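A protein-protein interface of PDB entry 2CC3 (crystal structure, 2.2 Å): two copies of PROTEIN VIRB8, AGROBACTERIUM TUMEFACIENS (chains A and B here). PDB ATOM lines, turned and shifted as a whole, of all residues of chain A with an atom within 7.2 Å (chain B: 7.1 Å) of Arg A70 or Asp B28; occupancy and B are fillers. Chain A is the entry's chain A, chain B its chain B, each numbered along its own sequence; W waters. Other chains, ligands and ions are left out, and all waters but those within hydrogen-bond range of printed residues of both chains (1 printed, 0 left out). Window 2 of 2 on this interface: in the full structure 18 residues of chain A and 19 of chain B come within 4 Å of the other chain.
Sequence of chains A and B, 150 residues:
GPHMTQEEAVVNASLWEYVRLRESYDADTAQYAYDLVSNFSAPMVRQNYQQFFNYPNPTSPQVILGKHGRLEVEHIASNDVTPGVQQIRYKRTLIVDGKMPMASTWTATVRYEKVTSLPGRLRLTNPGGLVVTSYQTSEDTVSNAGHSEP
Among the printed residues, merely in contact across the chains: Thr A29 with Thr B29.
Arg A70 touches one residue of chain B.
Asp B28 touches just these residues of chain A: Asp A26, Asp A28 and Arg A70.
Printed residues of chain B within 4 Å of Asp A28: Asp B26 (2.6 Å) and Asp B28 (2.7 Å).
Of the printed residues of chain B, Thr A29 touches Thr B29.
Of the printed residues of chain A, Thr B29 touches Thr A29 (3.5 Å).
Of the printed residues of chain B, Asp A26 touches Asp B28.
Ile A95 touches none of the printed residues of chain B.
Gly B66 touches none of the printed residues of chain A.
The nearest printed residue of chain B that does not touch Asp A26 is Thr B29 (4.7 Å).
The side-chain carboxylate of Asp B26 lies close to the side-chain carboxylate of Asp A28, at 2.6 Å.
The side-chain carboxylate (OD2) of Asp A28 lies close to the side-chain carboxylate (OD2) of Asp B28.
OD1 of Asp B28 is in salt-bridge range of NH1 of Arg A70 (2.9 Å).
OD1 of Asp A26 sits close to OD2 of Asp B28 (3.2 Å).
The side-chain carboxylate (OD2) of Asp A26 lies close to the backbone NH (N) of Asp A28 (3.4 Å).
The guanidinium group (NE) of Arg A70 is in salt-bridge range of the side-chain carboxylate (OD1) of Asp A26 (3.2 Å).
NH2 of Arg A70 lies within salt-bridge range of OE2 of Glu A72, at 3.7 Å.
The backbone carbonyl oxygen (O) of Arg A70 is in hydrogen-bond range of the backbone NH (N) of Ile A95.
The side-chain carboxylate (OD2) of Asp B26 sits close to the backbone NH (N) of Asp B28 (3.1 Å).
The backbone carbonyl oxygen (O) of Asp B26 lies within hydrogen-bond range of the side-chain hydroxyl (OG1) of Thr B29 (3.5 Å).
Among the printed residues, Asp or Glu carboxylates within 4 Å of a Lys or Arg side-chain nitrogen of the other chain: Arg A70 with Asp B28.
Water W1 lies within hydrogen-bond range of OD2 of Asp B26 (3.1 Å) and OD2 of Asp A28 (3.2 Å).
Asp A26 touches Asp B28, and with the chains exchanged Asp A28 touches Asp B26.
Asp A28 touches its own counterpart, Asp B28.
Thr A29 touches its own counterpart, Thr B29.
Positions printed for both chains: 25, 26, 27, 28, 29, 66 and 67.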
ATOM      1  N   SER A  24      -2.407 -24.352  -8.316  1.00  0.00           N
ATOM      2  CA  SER A  24      -2.273 -24.368  -9.771  1.00  0.00           C
ATOM      3  C   SER A  24      -3.557 -24.862 -10.405  1.00  0.00           C
ATOM      4  O   SER A  24      -4.365 -25.504  -9.730  1.00  0.00           O
ATOM      5  CB  SER A  24      -1.157 -25.327 -10.179  1.00  0.00           C
ATOM      6  OG  SER A  24       0.020 -24.621 -10.429  1.00  0.00           O
ATOM      7  N   TYR A  25      -3.748 -24.581 -11.692  1.00  0.00           N
ATOM      8  CA  TYR A  25      -4.847 -25.201 -12.458  1.00  0.00           C
ATOM      9  C   TYR A  25      -4.521 -25.375 -13.933  1.00  0.00           C
ATOM     10  O   TYR A  25      -4.111 -24.438 -14.619  1.00  0.00           O
ATOM     11  CB  TYR A  25      -6.184 -24.436 -12.369  1.00  0.00           C
ATOM     12  CG  TYR A  25      -7.258 -25.077 -13.254  1.00  0.00           C
ATOM     13  CD1 TYR A  25      -7.877 -26.265 -12.858  1.00  0.00           C
ATOM     14  CD2 TYR A  25      -7.614 -24.536 -14.490  1.00  0.00           C
ATOM     15  CE1 TYR A  25      -8.826 -26.886 -13.640  1.00  0.00           C
ATOM     16  CE2 TYR A  25      -8.577 -25.153 -15.283  1.00  0.00           C
ATOM     17  CZ  TYR A  25      -9.172 -26.336 -14.843  1.00  0.00           C
ATOM     18  OH  TYR A  25     -10.142 -26.994 -15.565  1.00  0.00           O
ATOM     19  N   ASP A  26      -4.759 -26.577 -14.426  1.00  0.00           N
ATOM     20  CA  ASP A  26      -4.604 -26.866 -15.847  1.00  0.00           C
ATOM     21  C   ASP A  26      -5.582 -27.995 -16.126  1.00  0.00           C
ATOM     22  O   ASP A  26      -5.505 -29.040 -15.488  1.00  0.00           O
ATOM     23  CB  ASP A  26      -3.151 -27.298 -16.110  1.00  0.00           C
ATOM     24  CG  ASP A  26      -2.841 -27.480 -17.582  1.00  0.00           C
ATOM     25  OD1 ASP A  26      -2.655 -26.478 -18.288  1.00  0.00           O
ATOM     26  OD2 ASP A  26      -2.751 -28.640 -18.043  1.00  0.00           O
ATOM     27  N   ALA A  27      -6.516 -27.798 -17.048  1.00  0.00           N
ATOM     28  CA  ALA A  27      -7.505 -28.859 -17.331  1.00  0.00           C
ATOM     29  C   ALA A  27      -6.866 -30.247 -17.584  1.00  0.00           C
ATOM     30  O   ALA A  27      -7.426 -31.280 -17.201  1.00  0.00           O
ATOM     31  CB  ALA A  27      -8.404 -28.445 -18.498  1.00  0.00           C
ATOM     32  N   ASP A  28      -5.686 -30.263 -18.210  1.00  0.00           N
ATOM     33  CA  ASP A  28      -4.963 -31.519 -18.452  1.00  0.00           C
ATOM     34  C   ASP A  28      -4.453 -32.191 -17.183  1.00  0.00           C
ATOM     35  O   ASP A  28      -4.384 -33.409 -17.130  1.00  0.00           O
ATOM     36  CB  ASP A  28      -3.792 -31.313 -19.419  1.00  0.00           C
ATOM     37  CG  ASP A  28      -4.251 -30.871 -20.796  1.00  0.00           C
ATOM     38  OD1 ASP A  28      -5.461 -31.018 -21.101  1.00  0.00           O
ATOM     39  OD2 ASP A  28      -3.406 -30.367 -21.576  1.00  0.00           O
ATOM     40  N   THR A  29      -4.082 -31.397 -16.175  1.00  0.00           N
ATOM     41  CA  THR A  29      -3.503 -31.910 -14.921  1.00  0.00           C
ATOM     42  C   THR A  29      -4.514 -31.920 -13.790  1.00  0.00           C
ATOM     43  O   THR A  29      -4.186 -32.278 -12.655  1.00  0.00           O
ATOM     44  CB  THR A  29      -2.333 -31.051 -14.452  1.00  0.00           C
ATOM     45  OG1 THR A  29      -2.797 -29.724 -14.185  1.00  0.00           O
ATOM     46  CG2 THR A  29      -1.216 -31.010 -15.485  1.00  0.00           C
ATOM     47  N   LEU A  65     -12.278 -21.295 -15.588  1.00  0.00           N
ATOM     48  CA  LEU A  65     -11.214 -21.317 -16.571  1.00  0.00           C
ATOM     49  C   LEU A  65     -11.347 -22.451 -17.580  1.00  0.00           C
ATOM     50  O   LEU A  65     -11.103 -22.239 -18.767  1.00  0.00           O
ATOM     51  CB  LEU A  65      -9.839 -21.324 -15.890  1.00  0.00           C
ATOM     52  CG  LEU A  65      -9.559 -20.150 -14.942  1.00  0.00           C
ATOM     53  CD1 LEU A  65      -8.336 -20.387 -14.097  1.00  0.00           C
ATOM     54  CD2 LEU A  65      -9.468 -18.815 -15.709  1.00  0.00           C
ATOM     55  N   GLY A  66     -11.764 -23.626 -17.114  1.00  0.00           N
ATOM     56  CA  GLY A  66     -11.924 -24.797 -17.967  1.00  0.00           C
ATOM     57  C   GLY A  66     -10.688 -25.076 -18.789  1.00  0.00           C
ATOM     58  O   GLY A  66      -9.570 -25.197 -18.270  1.00  0.00           O
ATOM     59  N   LYS A  67     -10.886 -25.129 -20.092  1.00  0.00           N
ATOM     60  CA  LYS A  67      -9.837 -25.493 -21.008  1.00  0.00           C
ATOM     61  C   LYS A  67      -9.142 -24.249 -21.529  1.00  0.00           C
ATOM     62  O   LYS A  67      -8.125 -24.356 -22.194  1.00  0.00           O
ATOM     63  CB  LYS A  67     -10.443 -26.325 -22.149  1.00  0.00           C
ATOM     64  CG  LYS A  67     -11.658 -27.180 -21.688  1.00  0.00           C
ATOM     65  CD  LYS A  67     -11.689 -28.624 -22.240  1.00  0.00           C
ATOM     66  CE  LYS A  67     -10.507 -29.472 -21.751  1.00  0.00           C
ATOM     67  NZ  LYS A  67      -9.250 -29.175 -22.515  1.00  0.00           N
ATOM     68  N   HIS A  68      -9.679 -23.072 -21.194  1.00  0.00           N
ATOM     69  CA  HIS A  68      -9.254 -21.777 -21.777  1.00  0.00           C
ATOM     70  C   HIS A  68      -8.378 -20.894 -20.888  1.00  0.00           C
ATOM     71  O   HIS A  68      -8.078 -19.740 -21.246  1.00  0.00           O
ATOM     72  CB  HIS A  68     -10.478 -20.953 -22.159  1.00  0.00           C
ATOM     73  CG  HIS A  68     -11.101 -21.361 -23.450  1.00  0.00           C
ATOM     74  ND1 HIS A  68     -11.351 -20.468 -24.464  1.00  0.00           N
ATOM     75  CD2 HIS A  68     -11.526 -22.569 -23.893  1.00  0.00           C
ATOM     76  CE1 HIS A  68     -11.906 -21.105 -25.477  1.00  0.00           C
ATOM     77  NE2 HIS A  68     -12.027 -22.381 -25.155  1.00  0.00           N
ATOM     78  N   GLY A  69      -8.002 -21.407 -19.726  1.00  0.00           N
ATOM     79  CA  GLY A  69      -7.199 -20.649 -18.797  1.00  0.00           C
ATOM     80  C   GLY A  69      -6.434 -21.571 -17.878  1.00  0.00           C
ATOM     81  O   GLY A  69      -6.733 -22.761 -17.771  1.00  0.00           O
ATOM     82  N   ARG A  70      -5.441 -21.003 -17.215  1.00  0.00           N
ATOM     83  CA  ARG A  70      -4.572 -21.734 -16.305  1.00  0.00           C
ATOM     84  C   ARG A  70      -4.161 -20.810 -15.173  1.00  0.00           C
ATOM     85  O   ARG A  70      -4.145 -19.593 -15.351  1.00  0.00           O
ATOM     86  CB  ARG A  70      -3.298 -22.177 -17.029  1.00  0.00           C
ATOM     87  CG  ARG A  70      -3.398 -23.487 -17.770  1.00  0.00           C
ATOM     88  CD  ARG A  70      -2.487 -23.486 -19.005  1.00  0.00           C
ATOM     89  NE  ARG A  70      -1.071 -23.696 -18.688  1.00  0.00           N
ATOM     90  CZ  ARG A  70      -0.202 -24.286 -19.514  1.00  0.00           C
ATOM     91  NH1 ARG A  70      -0.608 -24.726 -20.703  1.00  0.00           N
ATOM     92  NH2 ARG A  70       1.074 -24.432 -19.158  1.00  0.00           N
ATOM     93  N   LEU A  71      -3.806 -21.418 -14.041  1.00  0.00           N
ATOM     94  CA  LEU A  71      -3.200 -20.745 -12.909  1.00  0.00           C
ATOM     95  C   LEU A  71      -1.838 -21.372 -12.677  1.00  0.00           C
ATOM     96  O   LEU A  71      -1.728 -22.590 -12.576  1.00  0.00           O
ATOM     97  CB  LEU A  71      -4.080 -20.884 -11.650  1.00  0.00           C
ATOM     98  CG  LEU A  71      -5.447 -20.182 -11.564  1.00  0.00           C
ATOM     99  CD1 LEU A  71      -6.370 -20.796 -10.497  1.00  0.00           C
ATOM    100  CD2 LEU A  71      -5.342 -18.676 -11.351  1.00  0.00           C
ATOM    101  N   GLU A  72      -0.800 -20.530 -12.641  1.00  0.00           N
ATOM    102  CA  GLU A  72       0.561 -20.939 -12.312  1.00  0.00           C
ATOM    103  C   GLU A  72       1.073 -20.355 -10.980  1.00  0.00           C
ATOM    104  O   GLU A  72       0.710 -19.244 -10.593  1.00  0.00           O
ATOM    105  CB  GLU A  72       1.521 -20.596 -13.463  1.00  0.00           C
ATOM    106  CG  GLU A  72       1.402 -21.581 -14.614  1.00  0.00           C
ATOM    107  CD  GLU A  72       2.112 -21.122 -15.870  1.00  0.00           C
ATOM    108  OE1 GLU A  72       3.134 -20.390 -15.753  1.00  0.00           O
ATOM    109  OE2 GLU A  72       1.641 -21.499 -16.973  1.00  0.00           O
ATOM    110  N   ARG A  92       0.980 -16.084  -7.766  1.00  0.00           N
ATOM    111  CA  ARG A  92      -0.012 -16.810  -8.542  1.00  0.00           C
ATOM    112  C   ARG A  92      -0.390 -16.025  -9.798  1.00  0.00           C
ATOM    113  O   ARG A  92      -0.788 -14.872  -9.720  1.00  0.00           O
ATOM    114  CB  ARG A  92      -1.239 -17.077  -7.684  1.00  0.00           C
ATOM    115  CG  ARG A  92      -2.003 -18.352  -8.019  1.00  0.00           C
ATOM    116  CD  ARG A  92      -3.326 -17.990  -8.614  1.00  0.00           C
ATOM    117  NE  ARG A  92      -4.434 -18.629  -7.924  1.00  0.00           N
ATOM    118  CZ  ARG A  92      -5.611 -18.052  -7.674  1.00  0.00           C
ATOM    119  NH1 ARG A  92      -5.847 -16.785  -8.025  1.00  0.00           N
ATOM    120  NH2 ARG A  92      -6.555 -18.745  -7.047  1.00  0.00           N
ATOM    121  N   THR A  93      -0.260 -16.667 -10.954  1.00  0.00           N
ATOM    122  CA  THR A  93      -0.455 -16.014 -12.230  1.00  0.00           C
ATOM    123  C   THR A  93      -1.641 -16.645 -12.931  1.00  0.00           C
ATOM    124  O   THR A  93      -1.684 -17.869 -13.123  1.00  0.00           O
ATOM    125  CB  THR A  93       0.803 -16.174 -13.105  1.00  0.00           C
ATOM    126  OG1 THR A  93       1.964 -15.818 -12.342  1.00  0.00           O
ATOM    127  CG2 THR A  93       0.716 -15.313 -14.322  1.00  0.00           C
ATOM    128  N   LEU A  94      -2.601 -15.797 -13.290  1.00  0.00           N
ATOM    129  CA  LEU A  94      -3.744 -16.169 -14.109  1.00  0.00           C
ATOM    130  C   LEU A  94      -3.426 -15.892 -15.588  1.00  0.00           C
ATOM    131  O   LEU A  94      -3.128 -14.745 -15.964  1.00  0.00           O
ATOM    132  CB  LEU A  94      -4.988 -15.389 -13.663  1.00  0.00           C
ATOM    133  CG  LEU A  94      -6.216 -15.447 -14.565  1.00  0.00           C
ATOM    134  CD1 LEU A  94      -6.832 -16.825 -14.545  1.00  0.00           C
ATOM    135  CD2 LEU A  94      -7.233 -14.389 -14.149  1.00  0.00           C
ATOM    136  N   ILE A  95      -3.488 -16.947 -16.401  1.00  0.00           N
ATOM    137  CA  ILE A  95      -3.226 -16.857 -17.836  1.00  0.00           C
ATOM    138  C   ILE A  95      -4.483 -17.242 -18.611  1.00  0.00           C
ATOM    139  O   ILE A  95      -4.856 -18.405 -18.672  1.00  0.00           O
ATOM    140  CB  ILE A  95      -1.987 -17.727 -18.263  1.00  0.00           C
ATOM    141  CG1 ILE A  95      -0.742 -17.284 -17.477  1.00  0.00           C
ATOM    142  CG2 ILE A  95      -1.731 -17.641 -19.782  1.00  0.00           C
ATOM    143  CD1 ILE A  95       0.536 -18.019 -17.837  1.00  0.00           C
ATOM    144  N   VAL A  96      -5.143 -16.240 -19.183  1.00  0.00           N
ATOM    145  CA  VAL A  96      -6.340 -16.442 -20.000  1.00  0.00           C
ATOM    146  C   VAL A  96      -6.089 -15.976 -21.443  1.00  0.00           C
ATOM    147  O   VAL A  96      -5.103 -15.274 -21.706  1.00  0.00           O
ATOM    148  CB  VAL A  96      -7.590 -15.719 -19.394  1.00  0.00           C
ATOM    149  CG1 VAL A  96      -8.118 -16.473 -18.193  1.00  0.00           C
ATOM    150  CG2 VAL A  96      -7.267 -14.289 -19.006  1.00  0.00           C
ATOM    151  N   ASP A  97      -6.973 -16.385 -22.362  1.00  0.00           N
ATOM    152  CA  ASP A  97      -6.940 -15.974 -23.775  1.00  0.00           C
ATOM    153  C   ASP A  97      -7.152 -14.473 -23.927  1.00  0.00           C
ATOM    154  O   ASP A  97      -8.062 -13.920 -23.311  1.00  0.00           O
ATOM    155  CB  ASP A  97      -8.089 -16.636 -24.550  1.00  0.00           C
ATOM    156  CG  ASP A  97      -7.947 -18.137 -24.697  1.00  0.00           C
ATOM    157  OD1 ASP A  97      -6.817 -18.657 -24.829  1.00  0.00           O
ATOM    158  OD2 ASP A  97      -9.010 -18.797 -24.725  1.00  0.00           O
ATOM    159  N   MET A 102      -2.183 -12.016 -15.435  1.00  0.00           N
ATOM    160  CA  MET A 102      -2.509 -11.307 -14.192  1.00  0.00           C
ATOM    161  C   MET A 102      -1.955 -12.031 -12.980  1.00  0.00           C
ATOM    162  O   MET A 102      -2.235 -13.203 -12.776  1.00  0.00           O
ATOM    163  CB  MET A 102      -4.016 -11.156 -14.040  1.00  0.00           C
ATOM    164  CG  MET A 102      -4.603 -10.174 -15.005  1.00  0.00           C
ATOM    165  SD  MET A 102      -6.186 -10.786 -15.525  1.00  0.00           S
ATOM    166  CE  MET A 102      -5.724 -12.061 -16.708  1.00  0.00           C
ATOM    167  N   TYR B  25       3.772 -37.073 -21.648  1.00  0.00           N
ATOM    168  CA  TYR B  25       3.745 -35.878 -22.477  1.00  0.00           C
ATOM    169  C   TYR B  25       2.399 -35.174 -22.492  1.00  0.00           C
ATOM    170  O   TYR B  25       1.375 -35.780 -22.762  1.00  0.00           O
ATOM    171  CB  TYR B  25       4.201 -36.141 -23.916  1.00  0.00           C
ATOM    172  CG  TYR B  25       4.026 -34.900 -24.791  1.00  0.00           C
ATOM    173  CD1 TYR B  25       5.015 -33.940 -24.870  1.00  0.00           C
ATOM    174  CD2 TYR B  25       2.838 -34.676 -25.484  1.00  0.00           C
ATOM    175  CE1 TYR B  25       4.837 -32.799 -25.643  1.00  0.00           C
ATOM    176  CE2 TYR B  25       2.660 -33.556 -26.240  1.00  0.00           C
ATOM    177  CZ  TYR B  25       3.654 -32.623 -26.320  1.00  0.00           C
ATOM    178  OH  TYR B  25       3.466 -31.516 -27.096  1.00  0.00           O
ATOM    179  N   ASP B  26       2.428 -33.884 -22.207  1.00  0.00           N
ATOM    180  CA  ASP B  26       1.302 -33.007 -22.466  1.00  0.00           C
ATOM    181  C   ASP B  26       1.861 -31.654 -22.868  1.00  0.00           C
ATOM    182  O   ASP B  26       2.770 -31.129 -22.219  1.00  0.00           O
ATOM    183  CB  ASP B  26       0.423 -32.842 -21.224  1.00  0.00           C
ATOM    184  CG  ASP B  26      -0.951 -32.318 -21.566  1.00  0.00           C
ATOM    185  OD1 ASP B  26      -1.923 -32.977 -21.167  1.00  0.00           O
ATOM    186  OD2 ASP B  26      -1.063 -31.287 -22.271  1.00  0.00           O
ATOM    187  N   ALA B  27       1.343 -31.100 -23.951  1.00  0.00           N
ATOM    188  CA  ALA B  27       1.784 -29.777 -24.418  1.00  0.00           C
ATOM    189  C   ALA B  27       1.751 -28.691 -23.303  1.00  0.00           C
ATOM    190  O   ALA B  27       2.603 -27.787 -23.272  1.00  0.00           O
ATOM    191  CB  ALA B  27       0.956 -29.358 -25.635  1.00  0.00           C
ATOM    192  N   ASP B  28       0.786 -28.808 -22.389  1.00  0.00           N
ATOM    193  CA  ASP B  28       0.661 -27.899 -21.242  1.00  0.00           C
ATOM    194  C   ASP B  28       1.777 -28.071 -20.200  1.00  0.00           C
ATOM    195  O   ASP B  28       2.219 -27.119 -19.566  1.00  0.00           O
ATOM    196  CB  ASP B  28      -0.724 -28.061 -20.591  1.00  0.00           C
ATOM    197  CG  ASP B  28      -1.846 -27.521 -21.466  1.00  0.00           C
ATOM    198  OD1 ASP B  28      -1.537 -26.842 -22.462  1.00  0.00           O
ATOM    199  OD2 ASP B  28      -3.034 -27.766 -21.167  1.00  0.00           O
ATOM    200  N   THR B  29       2.242 -29.294 -20.021  1.00  0.00           N
ATOM    201  CA  THR B  29       3.284 -29.552 -19.029  1.00  0.00           C
ATOM    202  C   THR B  29       4.687 -29.766 -19.640  1.00  0.00           C
ATOM    203  O   THR B  29       5.659 -30.016 -18.903  1.00  0.00           O
ATOM    204  CB  THR B  29       2.898 -30.746 -18.141  1.00  0.00           C
ATOM    205  OG1 THR B  29       3.072 -31.960 -18.877  1.00  0.00           O
ATOM    206  CG2 THR B  29       1.443 -30.632 -17.658  1.00  0.00           C
ATOM    207  N   ALA B  30       4.800 -29.645 -20.972  1.00  0.00           N
ATOM    208  CA  ALA B  30       6.078 -29.841 -21.673  1.00  0.00           C
ATOM    209  C   ALA B  30       7.270 -29.046 -21.106  1.00  0.00           C
ATOM    210  O   ALA B  30       8.361 -29.617 -20.874  1.00  0.00           O
ATOM    211  CB  ALA B  30       5.923 -29.574 -23.178  1.00  0.00           C
ATOM    212  N   GLN B  31       7.071 -27.737 -20.892  1.00  0.00           N
ATOM    213  CA  GLN B  31       8.145 -26.861 -20.411  1.00  0.00           C
ATOM    214  C   GLN B  31       8.529 -27.099 -18.939  1.00  0.00           C
ATOM    215  O   GLN B  31       9.703 -27.067 -18.583  1.00  0.00           O
ATOM    216  CB  GLN B  31       7.777 -25.389 -20.632  1.00  0.00           C
ATOM    217  CG  GLN B  31       8.957 -24.412 -20.468  1.00  0.00           C
ATOM    218  CD  GLN B  31      10.038 -24.648 -21.508  1.00  0.00           C
ATOM    219  OE1 GLN B  31       9.776 -24.585 -22.712  1.00  0.00           O
ATOM    220  NE2 GLN B  31      11.255 -24.957 -21.051  1.00  0.00           N
ATOM    221  N   TYR B  32       7.528 -27.309 -18.092  1.00  0.00           N
ATOM    222  CA  TYR B  32       7.721 -27.685 -16.716  1.00  0.00           C
ATOM    223  C   TYR B  32       8.473 -29.023 -16.666  1.00  0.00           C
ATOM    224  O   TYR B  32       9.493 -29.130 -16.007  1.00  0.00           O
ATOM    225  CB  TYR B  32       6.352 -27.791 -16.006  1.00  0.00           C
ATOM    226  CG  TYR B  32       6.408 -28.453 -14.622  1.00  0.00           C
ATOM    227  CD1 TYR B  32       6.626 -27.691 -13.469  1.00  0.00           C
ATOM    228  CD2 TYR B  32       6.236 -29.834 -14.467  1.00  0.00           C
ATOM    229  CE1 TYR B  32       6.692 -28.280 -12.213  1.00  0.00           C
ATOM    230  CE2 TYR B  32       6.295 -30.431 -13.201  1.00  0.00           C
ATOM    231  CZ  TYR B  32       6.520 -29.643 -12.079  1.00  0.00           C
ATOM    232  OH  TYR B  32       6.584 -30.220 -10.813  1.00  0.00           O
ATOM    233  N   ALA B  33       7.976 -30.044 -17.371  1.00  0.00           N
ATOM    234  CA  ALA B  33       8.642 -31.356 -17.396  1.00  0.00           C
ATOM    235  C   ALA B  33      10.092 -31.251 -17.864  1.00  0.00           C
ATOM    236  O   ALA B  33      11.016 -31.713 -17.189  1.00  0.00           O
ATOM    237  CB  ALA B  33       7.869 -32.326 -18.269  1.00  0.00           C
ATOM    238  N   GLY B  66       1.888 -33.034 -30.141  1.00  0.00           N
ATOM    239  CA  GLY B  66       1.573 -31.614 -30.031  1.00  0.00           C
ATOM    240  C   GLY B  66       0.449 -31.354 -29.043  1.00  0.00           C
ATOM    241  O   GLY B  66       0.496 -31.791 -27.893  1.00  0.00           O
ATOM    242  N   LYS B  67      -0.581 -30.674 -29.517  1.00  0.00           N
ATOM    243  CA  LYS B  67      -1.696 -30.262 -28.680  1.00  0.00           C
ATOM    244  C   LYS B  67      -2.848 -31.260 -28.737  1.00  0.00           C
ATOM    245  O   LYS B  67      -3.788 -31.158 -27.953  1.00  0.00           O
ATOM    246  CB  LYS B  67      -2.160 -28.860 -29.094  1.00  0.00           C
ATOM    247  CG  LYS B  67      -1.093 -27.772 -28.907  1.00  0.00           C
ATOM    248  CD  LYS B  67      -1.678 -26.463 -28.403  1.00  0.00           C
ATOM    249  CE  LYS B  67      -2.170 -26.540 -26.920  1.00  0.00           C
ATOM    250  NZ  LYS B  67      -3.445 -27.332 -26.641  1.00  0.00           N
HETATM  251  O   HOH W   1      -2.673 -30.243 -24.694  1.00  0.00           O
